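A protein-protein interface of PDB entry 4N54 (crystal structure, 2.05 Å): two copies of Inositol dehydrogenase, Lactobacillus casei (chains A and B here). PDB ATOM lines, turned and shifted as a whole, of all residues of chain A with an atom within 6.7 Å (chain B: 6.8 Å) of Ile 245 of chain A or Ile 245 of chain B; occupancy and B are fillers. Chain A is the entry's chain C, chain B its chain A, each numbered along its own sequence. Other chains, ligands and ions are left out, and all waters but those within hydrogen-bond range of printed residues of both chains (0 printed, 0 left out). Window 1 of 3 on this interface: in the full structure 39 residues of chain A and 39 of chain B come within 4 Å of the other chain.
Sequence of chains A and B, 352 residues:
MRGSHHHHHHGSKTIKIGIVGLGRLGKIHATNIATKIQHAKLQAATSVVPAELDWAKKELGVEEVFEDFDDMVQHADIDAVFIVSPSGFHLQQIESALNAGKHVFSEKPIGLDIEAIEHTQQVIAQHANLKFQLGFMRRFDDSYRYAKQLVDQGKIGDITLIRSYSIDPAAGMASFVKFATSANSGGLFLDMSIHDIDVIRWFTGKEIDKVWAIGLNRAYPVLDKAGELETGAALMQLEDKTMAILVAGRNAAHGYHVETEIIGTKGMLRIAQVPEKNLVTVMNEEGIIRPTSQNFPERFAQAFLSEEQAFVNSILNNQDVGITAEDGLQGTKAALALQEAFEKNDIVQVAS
Of the 17 printed residues of chain A, 9 touch a printed residue of chain B.
Printed residues of chain A that touch a printed residue of chain B: Leu 161, Arg 163, Tyr 165, Ala 233, Leu 235, Met 243, Ile 245, Val 247 and Glu 261.
Hydrophobic or aromatic side chains of chain B within 4 Å of the printed part of chain A: Tyr 165, Ala 233, Leu 235, Met 243, Ile 245 and Val 247.
Among the printed residues, no Asp or Glu carboxylate lies within 4 Å of a Lys or Arg side-chain nitrogen of the other chain.
The guanidinium group (NE) of Arg 163 of chain B sits close to the side-chain hydroxyl (OH) of Tyr 165 of chain A (3.3 Å).
The side-chain hydroxyl of Tyr 165 of chain B lies within hydrogen-bond range of the guanidinium group of Arg 163 of chain A (3.2 Å).
OH of Tyr 165 of chain B lies within hydrogen-bond range of OE2 of Glu 261 of chain A (2.6 Å).
N of Ala 233 of chain B lies close to SD of Met 243 of chain A (3.8 Å).
The side-chain sulfur of Met 243 of chain B is in hydrogen-bond range of the backbone NH of Ala 233 of chain A (3.7 Å).
The side-chain carboxylate of Glu 261 of chain B sits at hydrogen-bond distance from the side-chain hydroxyl of Tyr 165 of chain A (2.8 Å).
Arg 163 of chain A touches its own counterpart, Arg 163 of chain B.
Leu 235 of chain A touches Ala 234 of chain B, but with the chains exchanged Ala 234 of chain A does not touch Leu 235 of chain B (4.02 Å).
Leu 235 of chain A touches its own counterpart, Leu 235 of chain B.
Ile 245 of chain A touches Val 247 of chain B, and with the chains exchanged Val 247 of chain A touches Ile 245 of chain B.
Of the 13 pairs that touch across the chains among the printed residues, 11 have their exchanged pair printed and touching as well.
The backbone NH of Ile 162 of chain B is in hydrogen-bond range of the backbone carbonyl oxygen of Met 243 of chain B (3.1 Å).
The side-chain carboxylate (OE1) of Glu 261 of chain B lies within salt-bridge range of the guanidinium group (NE) of Arg 163 of chain B, at 3.0 Å.
N of Ser 164 of chain B is in hydrogen-bond range of O of Ile 245 of chain B, 2.9 Å away.
The backbone carbonyl oxygen (O) of Ala 234 of chain B lies within hydrogen-bond range of the backbone NH (N) of Leu 246 of chain B, 2.9 Å away.
O of Ile 162 of chain A lies within hydrogen-bond range of N of Ile 245 of chain A.
The backbone NH of Val 247 of chain A is in hydrogen-bond range of the backbone carbonyl oxygen of Ser 164 of chain A (3.1 Å).
Of the printed residues of chain B, Ile 245 of chain A touches Ile 245 (3.8 Å) and Val 247 (3.7 Å).
Ile 245 of chain B touches just these residues of chain A: Ile 245 and Val 247.
Printed residues of chain B within 4 Å of Leu 235 of chain A: Ala 234 and Leu 235.
Printed residues of chain A within 4 Å of Leu 235 of chain B: Leu 235.
Of the printed residues of chain B, Val 247 of chain A touches Ile 245.
Leu 246 of chain B touches none of the printed residues of chain A.
Ser 164 of chain A touches none of the printed residues of chain B.
The nearest residue of chain B that does not touch Ile 245 of chain A is Tyr 165 of chain B (4.5 Å).
CG2 of Val 247 of chain B touches CD1 of Leu 161 of chain A, 3.8 Å away.
CD of Arg 163 of chain B touches CD of Arg 163 of chain A (3.6 Å).
CD2 of Leu 235 of chain A touches CA of Ala 234 of chain B, 3.8 Å away.
Leu 235 of chain B touches Leu 235 of chain A.
CD1 of Ile 245 of chain A touches CG2 of Ile 245 of chain B, 3.8 Å away.
CG2 of Val 247 of chain B touches CD1 of Ile 245 of chain A, at 3.7 Å.
Val 247 of chain A touches Ile 245 of chain B (CG2 to CD1, 3.8 Å).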
ATOM      1  N   LEU A 161       8.387   5.836  -4.730  1.00  0.00           N
ATOM      2  CA  LEU A 161       8.346   4.951  -3.580  1.00  0.00           C
ATOM      3  C   LEU A 161       6.992   4.999  -2.890  1.00  0.00           C
ATOM      4  O   LEU A 161       6.406   6.060  -2.743  1.00  0.00           O
ATOM      5  CB  LEU A 161       9.469   5.293  -2.603  1.00  0.00           C
ATOM      6  CG  LEU A 161       9.766   4.373  -1.415  1.00  0.00           C
ATOM      7  CD1 LEU A 161      11.166   4.554  -0.958  1.00  0.00           C
ATOM      8  CD2 LEU A 161       8.836   4.595  -0.260  1.00  0.00           C
ATOM      9  N   ILE A 162       6.504   3.832  -2.497  1.00  0.00           N
ATOM     10  CA  ILE A 162       5.344   3.719  -1.632  1.00  0.00           C
ATOM     11  C   ILE A 162       5.715   2.964  -0.351  1.00  0.00           C
ATOM     12  O   ILE A 162       6.277   1.879  -0.410  1.00  0.00           O
ATOM     13  CB  ILE A 162       4.175   3.025  -2.317  1.00  0.00           C
ATOM     14  CG1 ILE A 162       3.813   3.720  -3.616  1.00  0.00           C
ATOM     15  CG2 ILE A 162       2.959   2.970  -1.415  1.00  0.00           C
ATOM     16  CD1 ILE A 162       2.643   3.146  -4.270  1.00  0.00           C
ATOM     17  N   ARG A 163       5.423   3.560   0.795  1.00  0.00           N
ATOM     18  CA  ARG A 163       5.555   2.891   2.071  1.00  0.00           C
ATOM     19  C   ARG A 163       4.168   2.728   2.654  1.00  0.00           C
ATOM     20  O   ARG A 163       3.397   3.675   2.681  1.00  0.00           O
ATOM     21  CB  ARG A 163       6.451   3.680   3.025  1.00  0.00           C
ATOM     22  CG  ARG A 163       6.359   3.244   4.477  1.00  0.00           C
ATOM     23  CD  ARG A 163       7.210   4.064   5.400  1.00  0.00           C
ATOM     24  NE  ARG A 163       6.700   5.403   5.648  1.00  0.00           N
ATOM     25  CZ  ARG A 163       5.691   5.684   6.466  1.00  0.00           C
ATOM     26  NH1 ARG A 163       5.054   4.720   7.103  1.00  0.00           N
ATOM     27  NH2 ARG A 163       5.316   6.929   6.647  1.00  0.00           N
ATOM     28  N   SER A 164       3.838   1.520   3.086  1.00  0.00           N
ATOM     29  CA  SER A 164       2.521   1.263   3.627  1.00  0.00           C
ATOM     30  C   SER A 164       2.577   0.456   4.906  1.00  0.00           C
ATOM     31  O   SER A 164       3.189  -0.592   4.947  1.00  0.00           O
ATOM     32  CB  SER A 164       1.645   0.573   2.609  1.00  0.00           C
ATOM     33  OG  SER A 164       0.295   0.879   2.818  1.00  0.00           O
ATOM     34  N   TYR A 165       1.937   0.970   5.946  1.00  0.00           N
ATOM     35  CA  TYR A 165       1.895   0.324   7.247  1.00  0.00           C
ATOM     36  C   TYR A 165       0.499  -0.180   7.551  1.00  0.00           C
ATOM     37  O   TYR A 165      -0.468   0.544   7.407  1.00  0.00           O
ATOM     38  CB  TYR A 165       2.301   1.282   8.354  1.00  0.00           C
ATOM     39  CG  TYR A 165       3.762   1.572   8.532  1.00  0.00           C
ATOM     40  CD1 TYR A 165       4.679   1.369   7.527  1.00  0.00           C
ATOM     41  CD2 TYR A 165       4.227   2.052   9.722  1.00  0.00           C
ATOM     42  CE1 TYR A 165       6.001   1.642   7.721  1.00  0.00           C
ATOM     43  CE2 TYR A 165       5.531   2.322   9.915  1.00  0.00           C
ATOM     44  CZ  TYR A 165       6.424   2.118   8.923  1.00  0.00           C
ATOM     45  OH  TYR A 165       7.731   2.399   9.156  1.00  0.00           O
ATOM     46  N   ASP A 196      -2.407  -3.547   1.274  1.00  0.00           N
ATOM     47  CA  ASP A 196      -1.287  -2.716   0.890  1.00  0.00           C
ATOM     48  C   ASP A 196      -0.743  -3.043  -0.502  1.00  0.00           C
ATOM     49  O   ASP A 196      -0.359  -2.150  -1.231  1.00  0.00           O
ATOM     50  CB  ASP A 196      -0.184  -2.822   1.920  1.00  0.00           C
ATOM     51  CG  ASP A 196      -0.629  -2.369   3.278  1.00  0.00           C
ATOM     52  OD1 ASP A 196      -1.292  -1.334   3.361  1.00  0.00           O
ATOM     53  OD2 ASP A 196      -0.327  -3.070   4.250  1.00  0.00           O
ATOM     54  N   ILE A 200      -0.722  -0.510  -3.626  1.00  0.00           N
ATOM     55  CA  ILE A 200       0.466  -0.317  -4.427  1.00  0.00           C
ATOM     56  C   ILE A 200       0.215  -0.511  -5.927  1.00  0.00           C
ATOM     57  O   ILE A 200       0.628   0.299  -6.732  1.00  0.00           O
ATOM     58  CB  ILE A 200       1.590  -1.222  -3.933  1.00  0.00           C
ATOM     59  CG1 ILE A 200       2.107  -0.676  -2.609  1.00  0.00           C
ATOM     60  CG2 ILE A 200       2.700  -1.289  -4.939  1.00  0.00           C
ATOM     61  CD1 ILE A 200       2.973  -1.579  -1.873  1.00  0.00           C
ATOM     62  N   ALA A 233       8.424  -6.681   8.467  1.00  0.00           N
ATOM     63  CA  ALA A 233       8.826  -5.650   7.518  1.00  0.00           C
ATOM     64  C   ALA A 233       9.321  -6.252   6.207  1.00  0.00           C
ATOM     65  O   ALA A 233       9.917  -7.323   6.193  1.00  0.00           O
ATOM     66  CB  ALA A 233       9.873  -4.779   8.101  1.00  0.00           C
ATOM     67  N   ALA A 234       9.089  -5.545   5.114  1.00  0.00           N
ATOM     68  CA  ALA A 234       9.459  -6.030   3.804  1.00  0.00           C
ATOM     69  C   ALA A 234       9.927  -4.924   2.858  1.00  0.00           C
ATOM     70  O   ALA A 234       9.546  -3.766   2.993  1.00  0.00           O
ATOM     71  CB  ALA A 234       8.327  -6.790   3.198  1.00  0.00           C
ATOM     72  N   LEU A 235      10.772  -5.302   1.914  1.00  0.00           N
ATOM     73  CA  LEU A 235      11.198  -4.440   0.831  1.00  0.00           C
ATOM     74  C   LEU A 235      10.806  -5.111  -0.482  1.00  0.00           C
ATOM     75  O   LEU A 235      10.979  -6.308  -0.646  1.00  0.00           O
ATOM     76  CB  LEU A 235      12.698  -4.207   0.904  1.00  0.00           C
ATOM     77  CG  LEU A 235      13.358  -3.246  -0.071  1.00  0.00           C
ATOM     78  CD1 LEU A 235      12.679  -1.892  -0.045  1.00  0.00           C
ATOM     79  CD2 LEU A 235      14.785  -3.093   0.254  1.00  0.00           C
ATOM     80  N   MET A 236      10.252  -4.341  -1.407  1.00  0.00           N
ATOM     81  CA  MET A 236       9.813  -4.878  -2.681  1.00  0.00           C
ATOM     82  C   MET A 236      10.326  -4.016  -3.820  1.00  0.00           C
ATOM     83  O   MET A 236      10.448  -2.807  -3.679  1.00  0.00           O
ATOM     84  CB  MET A 236       8.289  -4.967  -2.743  1.00  0.00           C
ATOM     85  CG  MET A 236       7.637  -5.627  -1.536  1.00  0.00           C
ATOM     86  SD  MET A 236       5.956  -6.163  -1.750  1.00  0.00           S
ATOM     87  CE  MET A 236       5.125  -4.613  -1.795  1.00  0.00           C
ATOM     88  N   MET A 243      10.012   1.589  -6.027  1.00  0.00           N
ATOM     89  CA  MET A 243      10.295   1.003  -4.724  1.00  0.00           C
ATOM     90  C   MET A 243       9.063   0.905  -3.827  1.00  0.00           C
ATOM     91  O   MET A 243       8.160   1.726  -3.902  1.00  0.00           O
ATOM     92  CB  MET A 243      11.415   1.771  -4.026  1.00  0.00           C
ATOM     93  CG  MET A 243      12.688   1.863  -4.836  1.00  0.00           C
ATOM     94  SD  MET A 243      14.080   2.661  -4.074  1.00  0.00           S
ATOM     95  CE  MET A 243      13.721   4.357  -4.396  1.00  0.00           C
ATOM     96  N   ALA A 244       9.038  -0.125  -2.987  1.00  0.00           N
ATOM     97  CA  ALA A 244       7.974  -0.302  -2.015  1.00  0.00           C
ATOM     98  C   ALA A 244       8.437  -0.889  -0.668  1.00  0.00           C
ATOM     99  O   ALA A 244       9.273  -1.775  -0.612  1.00  0.00           O
ATOM    100  CB  ALA A 244       6.859  -1.092  -2.591  1.00  0.00           C
ATOM    101  N   ILE A 245       7.879  -0.355   0.408  1.00  0.00           N
ATOM    102  CA  ILE A 245       8.181  -0.764   1.767  1.00  0.00           C
ATOM    103  C   ILE A 245       6.889  -1.099   2.479  1.00  0.00           C
ATOM    104  O   ILE A 245       5.907  -0.375   2.378  1.00  0.00           O
ATOM    105  CB  ILE A 245       8.859   0.351   2.531  1.00  0.00           C
ATOM    106  CG1 ILE A 245      10.170   0.732   1.879  1.00  0.00           C
ATOM    107  CG2 ILE A 245       9.097  -0.041   3.963  1.00  0.00           C
ATOM    108  CD1 ILE A 245      10.725   1.991   2.388  1.00  0.00           C
ATOM    109  N   LEU A 246       6.884  -2.208   3.195  1.00  0.00           N
ATOM    110  CA  LEU A 246       5.731  -2.578   3.988  1.00  0.00           C
ATOM    111  C   LEU A 246       6.128  -2.823   5.437  1.00  0.00           C
ATOM    112  O   LEU A 246       7.220  -3.292   5.725  1.00  0.00           O
ATOM    113  CB  LEU A 246       5.083  -3.841   3.440  1.00  0.00           C
ATOM    114  CG  LEU A 246       4.544  -3.982   2.027  1.00  0.00           C
ATOM    115  CD1 LEU A 246       4.230  -5.425   1.811  1.00  0.00           C
ATOM    116  CD2 LEU A 246       3.317  -3.168   1.846  1.00  0.00           C
ATOM    117  N   VAL A 247       5.226  -2.497   6.340  1.00  0.00           N
ATOM    118  CA  VAL A 247       5.283  -3.000   7.692  1.00  0.00           C
ATOM    119  C   VAL A 247       3.928  -3.591   8.022  1.00  0.00           C
ATOM    120  O   VAL A 247       2.905  -3.010   7.713  1.00  0.00           O
ATOM    121  CB  VAL A 247       5.679  -1.933   8.704  1.00  0.00           C
ATOM    122  CG1 VAL A 247       5.475  -2.432  10.113  1.00  0.00           C
ATOM    123  CG2 VAL A 247       7.097  -1.534   8.499  1.00  0.00           C
ATOM    124  N   GLU A 261       2.162   6.036   2.512  1.00  0.00           N
ATOM    125  CA  GLU A 261       2.953   7.144   2.039  1.00  0.00           C
ATOM    126  C   GLU A 261       3.368   6.924   0.589  1.00  0.00           C
ATOM    127  O   GLU A 261       3.730   5.828   0.202  1.00  0.00           O
ATOM    128  CB  GLU A 261       4.168   7.304   2.926  1.00  0.00           C
ATOM    129  CG  GLU A 261       5.309   8.073   2.356  1.00  0.00           C
ATOM    130  CD  GLU A 261       6.575   7.850   3.139  1.00  0.00           C
ATOM    131  OE1 GLU A 261       6.652   8.281   4.297  1.00  0.00           O
ATOM    132  OE2 GLU A 261       7.493   7.235   2.598  1.00  0.00           O
ATOM    133  N   LEU B 161      11.705  -2.031  15.777  1.00  0.00           N
ATOM    134  CA  LEU B 161      11.963  -1.526  14.430  1.00  0.00           C
ATOM    135  C   LEU B 161      12.315  -0.051  14.423  1.00  0.00           C
ATOM    136  O   LEU B 161      11.713   0.739  15.127  1.00  0.00           O
ATOM    137  CB  LEU B 161      10.764  -1.785  13.528  1.00  0.00           C
ATOM    138  CG  LEU B 161      10.800  -1.456  12.039  1.00  0.00           C
ATOM    139  CD1 LEU B 161       9.847  -2.320  11.322  1.00  0.00           C
ATOM    140  CD2 LEU B 161      10.462  -0.021  11.754  1.00  0.00           C
ATOM    141  N   ILE B 162      13.300   0.298  13.611  1.00  0.00           N
ATOM    142  CA  ILE B 162      13.648   1.680  13.346  1.00  0.00           C
ATOM    143  C   ILE B 162      13.569   1.953  11.853  1.00  0.00           C
ATOM    144  O   ILE B 162      14.190   1.271  11.067  1.00  0.00           O
ATOM    145  CB  ILE B 162      15.052   2.032  13.828  1.00  0.00           C
ATOM    146  CG1 ILE B 162      15.150   1.909  15.344  1.00  0.00           C
ATOM    147  CG2 ILE B 162      15.410   3.425  13.416  1.00  0.00           C
ATOM    148  CD1 ILE B 162      16.507   2.084  15.875  1.00  0.00           C
ATOM    149  N   ARG B 163      12.775   2.938  11.473  1.00  0.00           N
ATOM    150  CA  ARG B 163      12.778   3.443  10.105  1.00  0.00           C
ATOM    151  C   ARG B 163      13.434   4.798  10.113  1.00  0.00           C
ATOM    152  O   ARG B 163      13.118   5.622  10.953  1.00  0.00           O
ATOM    153  CB  ARG B 163      11.362   3.542   9.572  1.00  0.00           C
ATOM    154  CG  ARG B 163      11.206   4.450   8.385  1.00  0.00           C
ATOM    155  CD  ARG B 163       9.785   4.538   7.915  1.00  0.00           C
ATOM    156  NE  ARG B 163       8.962   5.386   8.757  1.00  0.00           N
ATOM    157  CZ  ARG B 163       8.915   6.708   8.673  1.00  0.00           C
ATOM    158  NH1 ARG B 163       9.657   7.344   7.787  1.00  0.00           N
ATOM    159  NH2 ARG B 163       8.132   7.389   9.481  1.00  0.00           N
ATOM    160  N   SER B 164      14.361   5.031   9.200  1.00  0.00           N
ATOM    161  CA  SER B 164      15.017   6.317   9.132  1.00  0.00           C
ATOM    162  C   SER B 164      15.150   6.887   7.715  1.00  0.00           C
ATOM    163  O   SER B 164      15.628   6.225   6.820  1.00  0.00           O
ATOM    164  CB  SER B 164      16.362   6.247   9.831  1.00  0.00           C
ATOM    165  OG  SER B 164      16.627   7.423  10.550  1.00  0.00           O
ATOM    166  N   TYR B 165      14.699   8.118   7.531  1.00  0.00           N
ATOM    167  CA  TYR B 165      14.750   8.797   6.240  1.00  0.00           C
ATOM    168  C   TYR B 165      15.737   9.952   6.275  1.00  0.00           C
ATOM    169  O   TYR B 165      15.728  10.751   7.190  1.00  0.00           O
ATOM    170  CB  TYR B 165      13.392   9.370   5.867  1.00  0.00           C
ATOM    171  CG  TYR B 165      12.322   8.432   5.369  1.00  0.00           C
ATOM    172  CD1 TYR B 165      12.392   7.068   5.564  1.00  0.00           C
ATOM    173  CD2 TYR B 165      11.228   8.928   4.696  1.00  0.00           C
ATOM    174  CE1 TYR B 165      11.406   6.243   5.110  1.00  0.00           C
ATOM    175  CE2 TYR B 165      10.256   8.120   4.241  1.00  0.00           C
ATOM    176  CZ  TYR B 165      10.340   6.776   4.436  1.00  0.00           C
ATOM    177  OH  TYR B 165       9.349   5.976   3.967  1.00  0.00           O
ATOM    178  N   ASP B 196      22.126   7.442   9.611  1.00  0.00           N
ATOM    179  CA  ASP B 196      21.054   6.589  10.054  1.00  0.00           C
ATOM    180  C   ASP B 196      21.581   5.294  10.645  1.00  0.00           C
ATOM    181  O   ASP B 196      21.031   4.774  11.587  1.00  0.00           O
ATOM    182  CB  ASP B 196      20.128   6.281   8.901  1.00  0.00           C
ATOM    183  CG  ASP B 196      19.523   7.515   8.296  1.00  0.00           C
ATOM    184  OD1 ASP B 196      18.734   8.182   8.973  1.00  0.00           O
ATOM    185  OD2 ASP B 196      19.841   7.810   7.141  1.00  0.00           O
ATOM    186  N   ILE B 200      20.819   3.996  14.408  1.00  0.00           N
ATOM    187  CA  ILE B 200      20.393   2.641  14.682  1.00  0.00           C
ATOM    188  C   ILE B 200      21.303   1.960  15.697  1.00  0.00           C
ATOM    189  O   ILE B 200      20.824   1.306  16.591  1.00  0.00           O
ATOM    190  CB  ILE B 200      20.297   1.809  13.403  1.00  0.00           C
ATOM    191  CG1 ILE B 200      19.256   2.418  12.476  1.00  0.00           C
ATOM    192  CG2 ILE B 200      19.925   0.401  13.724  1.00  0.00           C
ATOM    193  CD1 ILE B 200      19.101   1.751  11.186  1.00  0.00           C
ATOM    194  N   ALA B 233      16.387   2.857  -1.119  1.00  0.00           N
ATOM    195  CA  ALA B 233      15.617   2.240  -0.054  1.00  0.00           C
ATOM    196  C   ALA B 233      16.284   0.943   0.376  1.00  0.00           C
ATOM    197  O   ALA B 233      16.892   0.277  -0.431  1.00  0.00           O
ATOM    198  CB  ALA B 233      14.238   1.983  -0.508  1.00  0.00           C
ATOM    199  N   ALA B 234      16.159   0.591   1.647  1.00  0.00           N
ATOM    200  CA  ALA B 234      16.848  -0.574   2.167  1.00  0.00           C
ATOM    201  C   ALA B 234      16.184  -1.227   3.368  1.00  0.00           C
ATOM    202  O   ALA B 234      15.646  -0.556   4.230  1.00  0.00           O
ATOM    203  CB  ALA B 234      18.253  -0.233   2.498  1.00  0.00           C
ATOM    204  N   LEU B 235      16.242  -2.546   3.398  1.00  0.00           N
ATOM    205  CA  LEU B 235      15.825  -3.336   4.542  1.00  0.00           C
ATOM    206  C   LEU B 235      17.061  -3.936   5.201  1.00  0.00           C
ATOM    207  O   LEU B 235      17.919  -4.477   4.528  1.00  0.00           O
ATOM    208  CB  LEU B 235      14.885  -4.436   4.093  1.00  0.00           C
ATOM    209  CG  LEU B 235      14.341  -5.408   5.120  1.00  0.00           C
ATOM    210  CD1 LEU B 235      13.614  -4.684   6.197  1.00  0.00           C
ATOM    211  CD2 LEU B 235      13.415  -6.357   4.465  1.00  0.00           C
ATOM    212  N   MET B 236      17.161  -3.795   6.516  1.00  0.00           N
ATOM    213  CA  MET B 236      18.270  -4.357   7.267  1.00  0.00           C
ATOM    214  C   MET B 236      17.780  -5.215   8.429  1.00  0.00           C
ATOM    215  O   MET B 236      16.754  -4.936   9.020  1.00  0.00           O
ATOM    216  CB  MET B 236      19.196  -3.270   7.788  1.00  0.00           C
ATOM    217  CG  MET B 236      19.554  -2.218   6.783  1.00  0.00           C
ATOM    218  SD  MET B 236      21.013  -1.279   7.165  1.00  0.00           S
ATOM    219  CE  MET B 236      20.490  -0.463   8.621  1.00  0.00           C
ATOM    220  N   MET B 243      14.521  -5.183  13.446  1.00  0.00           N
ATOM    221  CA  MET B 243      14.368  -4.760  12.058  1.00  0.00           C
ATOM    222  C   MET B 243      14.688  -3.273  11.798  1.00  0.00           C
ATOM    223  O   MET B 243      14.550  -2.431  12.676  1.00  0.00           O
ATOM    224  CB  MET B 243      12.966  -5.092  11.574  1.00  0.00           C
ATOM    225  CG  MET B 243      12.591  -6.556  11.696  1.00  0.00           C
ATOM    226  SD  MET B 243      10.907  -6.912  11.261  1.00  0.00           S
ATOM    227  CE  MET B 243      10.085  -6.221  12.656  1.00  0.00           C
ATOM    228  N   ALA B 244      15.131  -2.967  10.583  1.00  0.00           N
ATOM    229  CA  ALA B 244      15.437  -1.597  10.189  1.00  0.00           C
ATOM    230  C   ALA B 244      15.098  -1.292   8.728  1.00  0.00           C
ATOM    231  O   ALA B 244      15.263  -2.128   7.860  1.00  0.00           O
ATOM    232  CB  ALA B 244      16.835  -1.277  10.462  1.00  0.00           C
ATOM    233  N   ILE B 245      14.592  -0.091   8.484  1.00  0.00           N
ATOM    234  CA  ILE B 245      14.247   0.370   7.146  1.00  0.00           C
ATOM    235  C   ILE B 245      14.930   1.699   6.919  1.00  0.00           C
ATOM    236  O   ILE B 245      14.935   2.546   7.792  1.00  0.00           O
ATOM    237  CB  ILE B 245      12.741   0.549   6.975  1.00  0.00           C
ATOM    238  CG1 ILE B 245      12.019  -0.774   7.137  1.00  0.00           C
ATOM    239  CG2 ILE B 245      12.412   1.172   5.638  1.00  0.00           C
ATOM    240  CD1 ILE B 245      10.571  -0.645   7.362  1.00  0.00           C
ATOM    241  N   LEU B 246      15.545   1.859   5.762  1.00  0.00           N
ATOM    242  CA  LEU B 246      16.189   3.104   5.416  1.00  0.00           C
ATOM    243  C   LEU B 246      15.645   3.616   4.098  1.00  0.00           C
ATOM    244  O   LEU B 246      15.290   2.843   3.228  1.00  0.00           O
ATOM    245  CB  LEU B 246      17.696   2.936   5.304  1.00  0.00           C
ATOM    246  CG  LEU B 246      18.559   2.499   6.486  1.00  0.00           C
ATOM    247  CD1 LEU B 246      19.988   2.398   6.059  1.00  0.00           C
ATOM    248  CD2 LEU B 246      18.430   3.431   7.663  1.00  0.00           C
ATOM    249  N   VAL B 247      15.541   4.932   3.997  1.00  0.00           N
ATOM    250  CA  VAL B 247      15.389   5.620   2.733  1.00  0.00           C
ATOM    251  C   VAL B 247      16.334   6.806   2.744  1.00  0.00           C
ATOM    252  O   VAL B 247      16.458   7.490   3.737  1.00  0.00           O
ATOM    253  CB  VAL B 247      13.947   6.095   2.467  1.00  0.00           C
ATOM    254  CG1 VAL B 247      13.883   6.877   1.210  1.00  0.00           C
ATOM    255  CG2 VAL B 247      12.997   4.939   2.377  1.00  0.00           C
ATOM    256  N   GLU B 261      11.986   7.107  12.936  1.00  0.00           N
ATOM    257  CA  GLU B 261      10.903   6.495  13.666  1.00  0.00           C
ATOM    258  C   GLU B 261      11.378   5.270  14.438  1.00  0.00           C
ATOM    259  O   GLU B 261      12.110   4.436  13.915  1.00  0.00           O
ATOM    260  CB  GLU B 261       9.784   6.120  12.709  1.00  0.00           C
ATOM    261  CG  GLU B 261       8.873   5.004  13.161  1.00  0.00           C
ATOM    262  CD  GLU B 261       8.173   4.310  12.005  1.00  0.00           C
ATOM    263  OE1 GLU B 261       7.394   4.952  11.291  1.00  0.00           O
ATOM    264  OE2 GLU B 261       8.398   3.118  11.814  1.00  0.00           O
